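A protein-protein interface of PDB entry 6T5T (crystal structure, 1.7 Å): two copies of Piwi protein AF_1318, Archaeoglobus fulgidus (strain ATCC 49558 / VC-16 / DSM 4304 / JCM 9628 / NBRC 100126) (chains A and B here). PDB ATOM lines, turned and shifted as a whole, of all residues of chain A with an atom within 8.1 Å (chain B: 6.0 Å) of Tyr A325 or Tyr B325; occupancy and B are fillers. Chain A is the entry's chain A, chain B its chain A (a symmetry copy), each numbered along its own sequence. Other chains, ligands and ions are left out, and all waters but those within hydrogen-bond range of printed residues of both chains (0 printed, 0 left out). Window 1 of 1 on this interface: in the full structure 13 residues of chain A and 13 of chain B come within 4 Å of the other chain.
The backbone NH (N) of Lys A329 sits at hydrogen-bond distance from the backbone carbonyl oxygen (O) of Gly B316 (2.9 Å).
The backbone carbonyl oxygen (O) of Tyr A325 is in hydrogen-bond range of the side-chain hydroxyl (OG1) of Thr A340, 2.9 Å away. The backbone NH of Thr A340 sits at hydrogen-bond distance from the backbone carbonyl oxygen of Thr A328 (3.2 Å). The backbone NH of Thr B355 sits at hydrogen-bond distance from the backbone carbonyl oxygen of Val B314 (2.9 Å). OG1 of Thr B328 sits at hydrogen-bond distance from O of Pro B324, at 3.2 Å. The backbone carbonyl oxygen (O) of Tyr B325 sits at hydrogen-bond distance from the side-chain hydroxyl (OG1) of Thr B340, 2.9 Å away. N of Thr B340 lies within hydrogen-bond range of O of Thr B328 (3.2 Å).
Among the printed residues, pairs that only touch across the chains: Tyr A325 with Tyr B325 (3.3 Å), Thr A328 with Gly B316 (3.6 Å), Gly A316 with Thr B328 (3.6 Å), Tyr A325 with Thr B328 (3.7 Å), Thr A328 with Tyr B325 (3.7 Å), Lys A329 with Val B314 (3.8 Å), Thr A328 with Val B314 (3.9 Å) and Val A314 with Thr B328 (3.9 Å).
Of the printed residues of chain B, Tyr A325 touches Tyr B325 and Thr B328. Of the printed residues of chain A, Tyr B325 touches Tyr A325 and Thr A328. Printed residues of chain B within 4 Å of Val A314: Thr B328 (3.9 Å). Printed residues of chain A within 4 Å of Thr B328: Val A314 (3.9 Å), Gly A316 (3.6 Å) and Tyr A325 (3.7 Å). Of the printed residues of chain A, Val B314 touches Thr A328 and Lys A329. Printed residues of chain B within 4 Å of Lys A329: Val B314 and Gly B316. Of the printed residues of chain B, Thr A328 touches Val B314 (3.9 Å), Gly B316 (3.6 Å) and Tyr B325 (3.7 Å). Thr A355 touches none of the printed residues of chain B. The nearest residue of chain B that does not touch Tyr A325 is Pro B324 (4.6 Å). The nearest residue of chain A that does not touch Tyr B325 is Pro A324 (4.6 Å).
Hydrophobic or aromatic side chains of chain B within 4 Å of the printed part of chain A: Val B314 and Tyr B325. Of the 20 printed residues of chain A, 5 touch a printed residue of chain B. Among the printed residues, 9 pairs touch across the chains. Among the printed residues, no Asp or Glu carboxylate lies within 4 Å of a Lys or Arg side-chain nitrogen of the other chain.
Val A314 touches Thr B328, and with the chains exchanged Thr A328 touches Val B314. Gly A316 touches Thr B328, and with the chains exchanged Thr A328 touches Gly B316. Tyr B325 touches its own counterpart, Tyr A325. Tyr A325 touches Thr B328, and with the chains exchanged Thr A328 touches Tyr B325. Positions printed for both chains: 314, 316, 324, 325, 326, 327, 328, 340, 341, 342, 355 and 357. Of the 9 pairs that touch across the chains among the printed residues, 7 have their exchanged pair printed and touching as well.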
ATOM      1  N   PHE A 312      28.892  26.827  -9.613  1.00  0.00           N
ATOM      2  CA  PHE A 312      28.177  27.854 -10.365  1.00  0.00           C
ATOM      3  C   PHE A 312      26.911  28.226  -9.598  1.00  0.00           C
ATOM      4  O   PHE A 312      26.552  27.598  -8.590  1.00  0.00           O
ATOM      5  CB  PHE A 312      27.894  27.407 -11.827  1.00  0.00           C
ATOM      6  CG  PHE A 312      26.996  26.207 -11.961  1.00  0.00           C
ATOM      7  CD1 PHE A 312      25.637  26.342 -11.837  1.00  0.00           C
ATOM      8  CD2 PHE A 312      27.508  24.951 -12.297  1.00  0.00           C
ATOM      9  CE1 PHE A 312      24.774  25.250 -11.994  1.00  0.00           C
ATOM     10  CE2 PHE A 312      26.642  23.860 -12.470  1.00  0.00           C
ATOM     11  CZ  PHE A 312      25.286  24.018 -12.299  1.00  0.00           C
ATOM     12  N   TRP A 313      26.241  29.284 -10.044  1.00  0.00           N
ATOM     13  CA  TRP A 313      25.124  29.835  -9.295  1.00  0.00           C
ATOM     14  C   TRP A 313      23.939  30.021 -10.206  1.00  0.00           C
ATOM     15  O   TRP A 313      24.054  30.691 -11.242  1.00  0.00           O
ATOM     16  CB  TRP A 313      25.508  31.184  -8.661  1.00  0.00           C
ATOM     17  CG  TRP A 313      26.639  31.062  -7.715  1.00  0.00           C
ATOM     18  CD1 TRP A 313      26.545  30.917  -6.347  1.00  0.00           C
ATOM     19  CD2 TRP A 313      28.035  31.049  -8.030  1.00  0.00           C
ATOM     20  NE1 TRP A 313      27.800  30.811  -5.811  1.00  0.00           N
ATOM     21  CE2 TRP A 313      28.733  30.899  -6.812  1.00  0.00           C
ATOM     22  CE3 TRP A 313      28.774  31.144  -9.222  1.00  0.00           C
ATOM     23  CZ2 TRP A 313      30.117  30.833  -6.754  1.00  0.00           C
ATOM     24  CZ3 TRP A 313      30.171  31.087  -9.157  1.00  0.00           C
ATOM     25  CH2 TRP A 313      30.828  30.933  -7.920  1.00  0.00           C
ATOM     26  N   VAL A 314      22.788  29.485  -9.812  1.00  0.00           N
ATOM     27  CA  VAL A 314      21.570  29.764 -10.570  1.00  0.00           C
ATOM     28  C   VAL A 314      21.006  31.098 -10.087  1.00  0.00           C
ATOM     29  O   VAL A 314      20.610  31.238  -8.929  1.00  0.00           O
ATOM     30  CB  VAL A 314      20.543  28.641 -10.446  1.00  0.00           C
ATOM     31  CG1 VAL A 314      19.322  28.961 -11.301  1.00  0.00           C
ATOM     32  CG2 VAL A 314      21.167  27.300 -10.852  1.00  0.00           C
ATOM     33  N   MET A 315      20.985  32.098 -10.973  1.00  0.00           N
ATOM     34  CA  MET A 315      20.427  33.394 -10.613  1.00  0.00           C
ATOM     35  C   MET A 315      18.916  33.409 -10.747  1.00  0.00           C
ATOM     36  O   MET A 315      18.313  34.484 -10.734  1.00  0.00           O
ATOM     37  CB  MET A 315      21.053  34.510 -11.467  1.00  0.00           C
ATOM     38  CG  MET A 315      22.557  34.328 -11.729  1.00  0.00           C
ATOM     39  SD  MET A 315      23.081  35.438 -13.050  1.00  0.00           S
ATOM     40  CE  MET A 315      23.470  36.907 -12.111  1.00  0.00           C
ATOM     41  N   GLY A 316      18.310  32.230 -10.857  1.00  0.00           N
ATOM     42  CA  GLY A 316      16.905  32.074 -11.179  1.00  0.00           C
ATOM     43  C   GLY A 316      16.714  31.756 -12.654  1.00  0.00           C
ATOM     44  O   GLY A 316      17.439  32.279 -13.503  1.00  0.00           O
ATOM     45  N   PRO A 324      14.616  24.484  -8.056  1.00  0.00           N
ATOM     46  CA  PRO A 324      14.538  23.042  -7.756  1.00  0.00           C
ATOM     47  C   PRO A 324      15.634  22.192  -8.436  1.00  0.00           C
ATOM     48  O   PRO A 324      15.361  21.430  -9.364  1.00  0.00           O
ATOM     49  CB  PRO A 324      13.148  22.650  -8.278  1.00  0.00           C
ATOM     50  CG  PRO A 324      12.771  23.734  -9.260  1.00  0.00           C
ATOM     51  CD  PRO A 324      13.387  24.984  -8.697  1.00  0.00           C
ATOM     52  N   TYR A 325      16.869  22.328  -7.964  1.00  0.00           N
ATOM     53  CA  TYR A 325      17.991  21.526  -8.444  1.00  0.00           C
ATOM     54  C   TYR A 325      18.388  20.449  -7.436  1.00  0.00           C
ATOM     55  O   TYR A 325      19.405  19.767  -7.619  1.00  0.00           O
ATOM     56  CB  TYR A 325      19.159  22.454  -8.798  1.00  0.00           C
ATOM     57  CG  TYR A 325      18.662  23.522  -9.760  1.00  0.00           C
ATOM     58  CD1 TYR A 325      18.105  24.711  -9.291  1.00  0.00           C
ATOM     59  CD2 TYR A 325      18.674  23.307 -11.133  1.00  0.00           C
ATOM     60  CE1 TYR A 325      17.595  25.659 -10.154  1.00  0.00           C
ATOM     61  CE2 TYR A 325      18.175  24.265 -12.007  1.00  0.00           C
ATOM     62  CZ  TYR A 325      17.635  25.435 -11.512  1.00  0.00           C
ATOM     63  OH  TYR A 325      17.135  26.388 -12.376  1.00  0.00           O
ATOM     64  N   GLU A 326      17.590  20.265  -6.390  1.00  0.00           N
ATOM     65  CA  GLU A 326      17.847  19.236  -5.384  1.00  0.00           C
ATOM     66  C   GLU A 326      17.512  17.880  -5.988  1.00  0.00           C
ATOM     67  O   GLU A 326      16.340  17.516  -6.123  1.00  0.00           O
ATOM     68  CB  GLU A 326      17.032  19.513  -4.129  1.00  0.00           C
ATOM     69  CG  GLU A 326      17.378  18.634  -2.943  1.00  0.00           C
ATOM     70  CD  GLU A 326      18.784  18.888  -2.411  1.00  0.00           C
ATOM     71  OE1 GLU A 326      19.231  20.052  -2.412  1.00  0.00           O
ATOM     72  OE2 GLU A 326      19.446  17.921  -2.004  1.00  0.00           O
ATOM     73  N   GLY A 327      18.544  17.136  -6.371  1.00  0.00           N
ATOM     74  CA  GLY A 327      18.377  15.866  -7.047  1.00  0.00           C
ATOM     75  C   GLY A 327      18.406  15.916  -8.568  1.00  0.00           C
ATOM     76  O   GLY A 327      18.206  14.874  -9.202  1.00  0.00           O
ATOM     77  N   THR A 328      18.659  17.076  -9.170  1.00  0.00           N
ATOM     78  CA  THR A 328      18.575  17.179 -10.628  1.00  0.00           C
ATOM     79  C   THR A 328      19.761  16.512 -11.324  1.00  0.00           C
ATOM     80  O   THR A 328      20.917  16.668 -10.918  1.00  0.00           O
ATOM     81  CB  THR A 328      18.469  18.645 -11.064  1.00  0.00           C
ATOM     82  OG1 THR A 328      17.189  19.149 -10.671  1.00  0.00           O
ATOM     83  CG2 THR A 328      18.615  18.768 -12.601  1.00  0.00           C
ATOM     84  N   LYS A 329      19.457  15.766 -12.381  1.00  0.00           N
ATOM     85  CA  LYS A 329      20.425  15.023 -13.175  1.00  0.00           C
ATOM     86  C   LYS A 329      20.490  15.596 -14.583  1.00  0.00           C
ATOM     87  O   LYS A 329      19.443  15.771 -15.222  1.00  0.00           O
ATOM     88  CB  LYS A 329      20.020  13.550 -13.257  1.00  0.00           C
ATOM     89  CG  LYS A 329      19.810  12.909 -11.891  1.00  0.00           C
ATOM     90  CD  LYS A 329      19.345  11.463 -12.036  1.00  0.00           C
ATOM     91  CE  LYS A 329      17.874  11.391 -12.380  1.00  0.00           C
ATOM     92  NZ  LYS A 329      17.078  10.913 -11.248  1.00  0.00           N
ATOM     93  N   VAL A 330      21.706  15.833 -15.079  1.00  0.00           N
ATOM     94  CA  VAL A 330      21.946  16.422 -16.401  1.00  0.00           C
ATOM     95  C   VAL A 330      22.703  15.406 -17.237  1.00  0.00           C
ATOM     96  O   VAL A 330      23.722  14.869 -16.795  1.00  0.00           O
ATOM     97  CB  VAL A 330      22.759  17.727 -16.281  1.00  0.00           C
ATOM     98  CG1 VAL A 330      23.166  18.260 -17.702  1.00  0.00           C
ATOM     99  CG2 VAL A 330      21.986  18.759 -15.473  1.00  0.00           C
ATOM    100  N   LEU A 339      25.528  15.908 -11.698  1.00  0.00           N
ATOM    101  CA  LEU A 339      24.570  15.986 -10.605  1.00  0.00           C
ATOM    102  C   LEU A 339      24.670  17.377  -9.991  1.00  0.00           C
ATOM    103  O   LEU A 339      25.756  17.784  -9.566  1.00  0.00           O
ATOM    104  CB  LEU A 339      24.866  14.922  -9.531  1.00  0.00           C
ATOM    105  CG  LEU A 339      24.195  13.572  -9.696  1.00  0.00           C
ATOM    106  CD1 LEU A 339      24.721  12.583  -8.635  1.00  0.00           C
ATOM    107  CD2 LEU A 339      22.670  13.655  -9.559  1.00  0.00           C
ATOM    108  N   THR A 340      23.562  18.129  -9.980  1.00  0.00           N
ATOM    109  CA  THR A 340      23.589  19.505  -9.465  1.00  0.00           C
ATOM    110  C   THR A 340      23.379  19.483  -7.958  1.00  0.00           C
ATOM    111  O   THR A 340      22.315  19.811  -7.447  1.00  0.00           O
ATOM    112  CB  THR A 340      22.538  20.397 -10.120  1.00  0.00           C
ATOM    113  OG1 THR A 340      21.237  19.873  -9.886  1.00  0.00           O
ATOM    114  CG2 THR A 340      22.774  20.498 -11.583  1.00  0.00           C
ATOM    115  N   LEU A 341      24.444  19.164  -7.239  1.00  0.00           N
ATOM    116  CA  LEU A 341      24.368  19.140  -5.783  1.00  0.00           C
ATOM    117  C   LEU A 341      24.376  20.565  -5.236  1.00  0.00           C
ATOM    118  O   LEU A 341      25.151  21.422  -5.688  1.00  0.00           O
ATOM    119  CB  LEU A 341      25.542  18.323  -5.210  1.00  0.00           C
ATOM    120  CG  LEU A 341      25.664  16.867  -5.691  1.00  0.00           C
ATOM    121  CD1 LEU A 341      26.847  16.130  -5.043  1.00  0.00           C
ATOM    122  CD2 LEU A 341      24.374  16.049  -5.448  1.00  0.00           C
ATOM    123  N   LEU A 342      23.492  20.835  -4.283  1.00  0.00           N
ATOM    124  CA  LEU A 342      23.442  22.151  -3.666  1.00  0.00           C
ATOM    125  C   LEU A 342      24.615  22.324  -2.711  1.00  0.00           C
ATOM    126  O   LEU A 342      25.053  21.370  -2.062  1.00  0.00           O
ATOM    127  CB  LEU A 342      22.122  22.348  -2.918  1.00  0.00           C
ATOM    128  CG  LEU A 342      20.990  22.925  -3.771  1.00  0.00           C
ATOM    129  CD1 LEU A 342      20.616  21.980  -4.911  1.00  0.00           C
ATOM    130  CD2 LEU A 342      19.779  23.251  -2.934  1.00  0.00           C
ATOM    131  N   THR A 355      21.288  30.757  -6.182  1.00  0.00           N
ATOM    132  CA  THR A 355      21.339  29.407  -5.616  1.00  0.00           C
ATOM    133  C   THR A 355      22.687  28.779  -5.918  1.00  0.00           C
ATOM    134  O   THR A 355      22.980  28.521  -7.103  1.00  0.00           O
ATOM    135  CB  THR A 355      20.225  28.535  -6.195  1.00  0.00           C
ATOM    136  OG1 THR A 355      18.948  29.056  -5.809  1.00  0.00           O
ATOM    137  CG2 THR A 355      20.362  27.091  -5.690  1.00  0.00           C
ATOM    138  N   PRO A 356      23.530  28.488  -4.910  1.00  0.00           N
ATOM    139  CA  PRO A 356      24.846  27.908  -5.189  1.00  0.00           C
ATOM    140  C   PRO A 356      24.730  26.415  -5.463  1.00  0.00           C
ATOM    141  O   PRO A 356      24.092  25.670  -4.706  1.00  0.00           O
ATOM    142  CB  PRO A 356      25.652  28.178  -3.901  1.00  0.00           C
ATOM    143  CG  PRO A 356      24.857  29.207  -3.170  1.00  0.00           C
ATOM    144  CD  PRO A 356      23.433  28.939  -3.514  1.00  0.00           C
ATOM    145  N   ILE A 357      25.375  25.987  -6.545  1.00  0.00           N
ATOM    146  CA  ILE A 357      25.457  24.593  -6.958  1.00  0.00           C
ATOM    147  C   ILE A 357      26.910  24.166  -6.866  1.00  0.00           C
ATOM    148  O   ILE A 357      27.805  24.905  -7.301  1.00  0.00           O
ATOM    149  CB  ILE A 357      24.951  24.429  -8.404  1.00  0.00           C
ATOM    150  CG1 ILE A 357      23.534  24.970  -8.525  1.00  0.00           C
ATOM    151  CG2 ILE A 357      25.152  23.003  -8.920  1.00  0.00           C
ATOM    152  CD1 ILE A 357      22.511  24.254  -7.674  1.00  0.00           C
ATOM    153  N   TYR A 386      23.293  10.553  -5.483  1.00  0.00           N
ATOM    154  CA  TYR A 386      22.610  11.615  -4.759  1.00  0.00           C
ATOM    155  C   TYR A 386      22.256  11.188  -3.319  1.00  0.00           C
ATOM    156  O   TYR A 386      22.516  11.937  -2.382  1.00  0.00           O
ATOM    157  CB  TYR A 386      21.358  12.053  -5.553  1.00  0.00           C
ATOM    158  CG  TYR A 386      20.469  12.948  -4.740  1.00  0.00           C
ATOM    159  CD1 TYR A 386      20.809  14.280  -4.528  1.00  0.00           C
ATOM    160  CD2 TYR A 386      19.330  12.452  -4.142  1.00  0.00           C
ATOM    161  CE1 TYR A 386      19.993  15.109  -3.772  1.00  0.00           C
ATOM    162  CE2 TYR A 386      18.523  13.249  -3.375  1.00  0.00           C
ATOM    163  CZ  TYR A 386      18.849  14.576  -3.195  1.00  0.00           C
ATOM    164  OH  TYR A 386      17.998  15.334  -2.417  1.00  0.00           O
ATOM    165  N   VAL B 314      18.207  17.773 -19.522  1.00  0.00           N
ATOM    166  CA  VAL B 314      17.834  17.584 -18.122  1.00  0.00           C
ATOM    167  C   VAL B 314      16.966  16.331 -18.028  1.00  0.00           C
ATOM    168  O   VAL B 314      15.868  16.276 -18.583  1.00  0.00           O
ATOM    169  CB  VAL B 314      17.122  18.806 -17.544  1.00  0.00           C
ATOM    170  CG1 VAL B 314      16.809  18.572 -16.071  1.00  0.00           C
ATOM    171  CG2 VAL B 314      17.980  20.063 -17.737  1.00  0.00           C
ATOM    172  N   GLY B 316      15.461  15.437 -15.563  1.00  0.00           N
ATOM    173  CA  GLY B 316      14.694  15.716 -14.365  1.00  0.00           C
ATOM    174  C   GLY B 316      15.609  15.993 -13.182  1.00  0.00           C
ATOM    175  O   GLY B 316      16.664  15.369 -13.051  1.00  0.00           O
ATOM    176  N   PRO B 324      11.632  23.609 -15.329  1.00  0.00           N
ATOM    177  CA  PRO B 324      11.509  25.062 -15.549  1.00  0.00           C
ATOM    178  C   PRO B 324      12.846  25.774 -15.850  1.00  0.00           C
ATOM    179  O   PRO B 324      13.367  26.523 -15.021  1.00  0.00           O
ATOM    180  CB  PRO B 324      10.914  25.566 -14.225  1.00  0.00           C
ATOM    181  CG  PRO B 324      11.219  24.487 -13.214  1.00  0.00           C
ATOM    182  CD  PRO B 324      11.149  23.206 -13.997  1.00  0.00           C
ATOM    183  N   TYR B 325      13.390  25.537 -17.040  1.00  0.00           N
ATOM    184  CA  TYR B 325      14.602  26.208 -17.501  1.00  0.00           C
ATOM    185  C   TYR B 325      14.294  27.279 -18.545  1.00  0.00           C
ATOM    186  O   TYR B 325      15.214  27.852 -19.144  1.00  0.00           O
ATOM    187  CB  TYR B 325      15.593  25.157 -18.017  1.00  0.00           C
ATOM    188  CG  TYR B 325      15.800  24.106 -16.938  1.00  0.00           C
ATOM    189  CD1 TYR B 325      14.961  22.996 -16.844  1.00  0.00           C
ATOM    190  CD2 TYR B 325      16.779  24.265 -15.966  1.00  0.00           C
ATOM    191  CE1 TYR B 325      15.101  22.069 -15.832  1.00  0.00           C
ATOM    192  CE2 TYR B 325      16.934  23.327 -14.953  1.00  0.00           C
ATOM    193  CZ  TYR B 325      16.091  22.234 -14.890  1.00  0.00           C
ATOM    194  OH  TYR B 325      16.238  21.302 -13.884  1.00  0.00           O
ATOM    195  N   GLU B 326      13.017  27.581 -18.754  1.00  0.00           N
ATOM    196  CA  GLU B 326      12.605  28.619 -19.697  1.00  0.00           C
ATOM    197  C   GLU B 326      12.915  29.976 -19.083  1.00  0.00           C
ATOM    198  O   GLU B 326      12.205  30.447 -18.188  1.00  0.00           O
ATOM    199  CB  GLU B 326      11.127  28.472 -20.027  1.00  0.00           C
ATOM    200  CG  GLU B 326      10.639  29.359 -21.155  1.00  0.00           C
ATOM    201  CD  GLU B 326      11.252  28.991 -22.502  1.00  0.00           C
ATOM    202  OE1 GLU B 326      11.459  27.789 -22.765  1.00  0.00           O
ATOM    203  OE2 GLU B 326      11.537  29.904 -23.292  1.00  0.00           O
ATOM    204  N   GLY B 327      13.990  30.601 -19.550  1.00  0.00           N
ATOM    205  CA  GLY B 327      14.461  31.854 -18.997  1.00  0.00           C
ATOM    206  C   GLY B 327      15.530  31.742 -17.919  1.00  0.00           C
ATOM    207  O   GLY B 327      15.927  32.773 -17.363  1.00  0.00           O
ATOM    208  N   THR B 328      16.015  30.539 -17.614  1.00  0.00           N
ATOM    209  CA  THR B 328      16.954  30.388 -16.501  1.00  0.00           C
ATOM    210  C   THR B 328      18.349  30.909 -16.846  1.00  0.00           C
ATOM    211  O   THR B 328      18.880  30.658 -17.933  1.00  0.00           O
ATOM    212  CB  THR B 328      17.037  28.924 -16.057  1.00  0.00           C
ATOM    213  OG1 THR B 328      15.801  28.562 -15.434  1.00  0.00           O
ATOM    214  CG2 THR B 328      18.194  28.727 -15.045  1.00  0.00           C
ATOM    215  N   THR B 340      19.980  28.985 -20.382  1.00  0.00           N
ATOM    216  CA  THR B 340      19.510  27.634 -20.718  1.00  0.00           C
ATOM    217  C   THR B 340      18.320  27.735 -21.660  1.00  0.00           C
ATOM    218  O   THR B 340      17.173  27.533 -21.279  1.00  0.00           O
ATOM    219  CB  THR B 340      19.124  26.823 -19.483  1.00  0.00           C
ATOM    220  OG1 THR B 340      18.083  27.479 -18.772  1.00  0.00           O
ATOM    221  CG2 THR B 340      20.296  26.642 -18.588  1.00  0.00           C
ATOM    222  N   LEU B 341      18.615  27.976 -22.927  1.00  0.00           N
ATOM    223  CA  LEU B 341      17.555  28.065 -23.926  1.00  0.00           C
ATOM    224  C   LEU B 341      17.044  26.669 -24.269  1.00  0.00           C
ATOM    225  O   LEU B 341      17.828  25.724 -24.447  1.00  0.00           O
ATOM    226  CB  LEU B 341      18.078  28.786 -25.183  1.00  0.00           C
ATOM    227  CG  LEU B 341      18.639  30.203 -24.978  1.00  0.00           C
ATOM    228  CD1 LEU B 341      19.109  30.847 -26.292  1.00  0.00           C
ATOM    229  CD2 LEU B 341      17.627  31.152 -24.292  1.00  0.00           C
ATOM    230  N   LEU B 342      15.725  26.524 -24.334  1.00  0.00           N
ATOM    231  CA  LEU B 342      15.136  25.243 -24.693  1.00  0.00           C
ATOM    232  C   LEU B 342      15.297  24.995 -26.186  1.00  0.00           C
ATOM    233  O   LEU B 342      15.253  25.927 -26.994  1.00  0.00           O
ATOM    234  CB  LEU B 342      13.654  25.205 -24.310  1.00  0.00           C
ATOM    235  CG  LEU B 342      13.379  24.708 -22.890  1.00  0.00           C
ATOM    236  CD1 LEU B 342      13.992  25.640 -21.847  1.00  0.00           C
ATOM    237  CD2 LEU B 342      11.901  24.535 -22.642  1.00  0.00           C
ATOM    238  N   THR B 355      14.499  16.795 -21.051  1.00  0.00           N
ATOM    239  CA  THR B 355      14.275  18.156 -21.547  1.00  0.00           C
ATOM    240  C   THR B 355      15.510  18.638 -22.287  1.00  0.00           C
ATOM    241  O   THR B 355      16.565  18.819 -21.646  1.00  0.00           O
ATOM    242  CB  THR B 355      13.963  19.109 -20.393  1.00  0.00           C
ATOM    243  OG1 THR B 355      12.732  18.729 -19.768  1.00  0.00           O
ATOM    244  CG2 THR B 355      13.852  20.551 -20.908  1.00  0.00           C
ATOM    245  N   ILE B 357      18.137  21.128 -23.805  1.00  0.00           N
ATOM    246  CA  ILE B 357      18.618  22.491 -23.618  1.00  0.00           C
ATOM    247  C   ILE B 357      19.635  22.778 -24.706  1.00  0.00           C
ATOM    248  O   ILE B 357      20.504  21.939 -24.984  1.00  0.00           O
ATOM    249  CB  ILE B 357      19.272  22.646 -22.233  1.00  0.00           C
ATOM    250  CG1 ILE B 357      18.289  22.241 -21.143  1.00  0.00           C
ATOM    251  CG2 ILE B 357      19.911  24.024 -22.055  1.00  0.00           C
ATOM    252  CD1 ILE B 357      17.038  23.086 -21.077  1.00  0.00           C
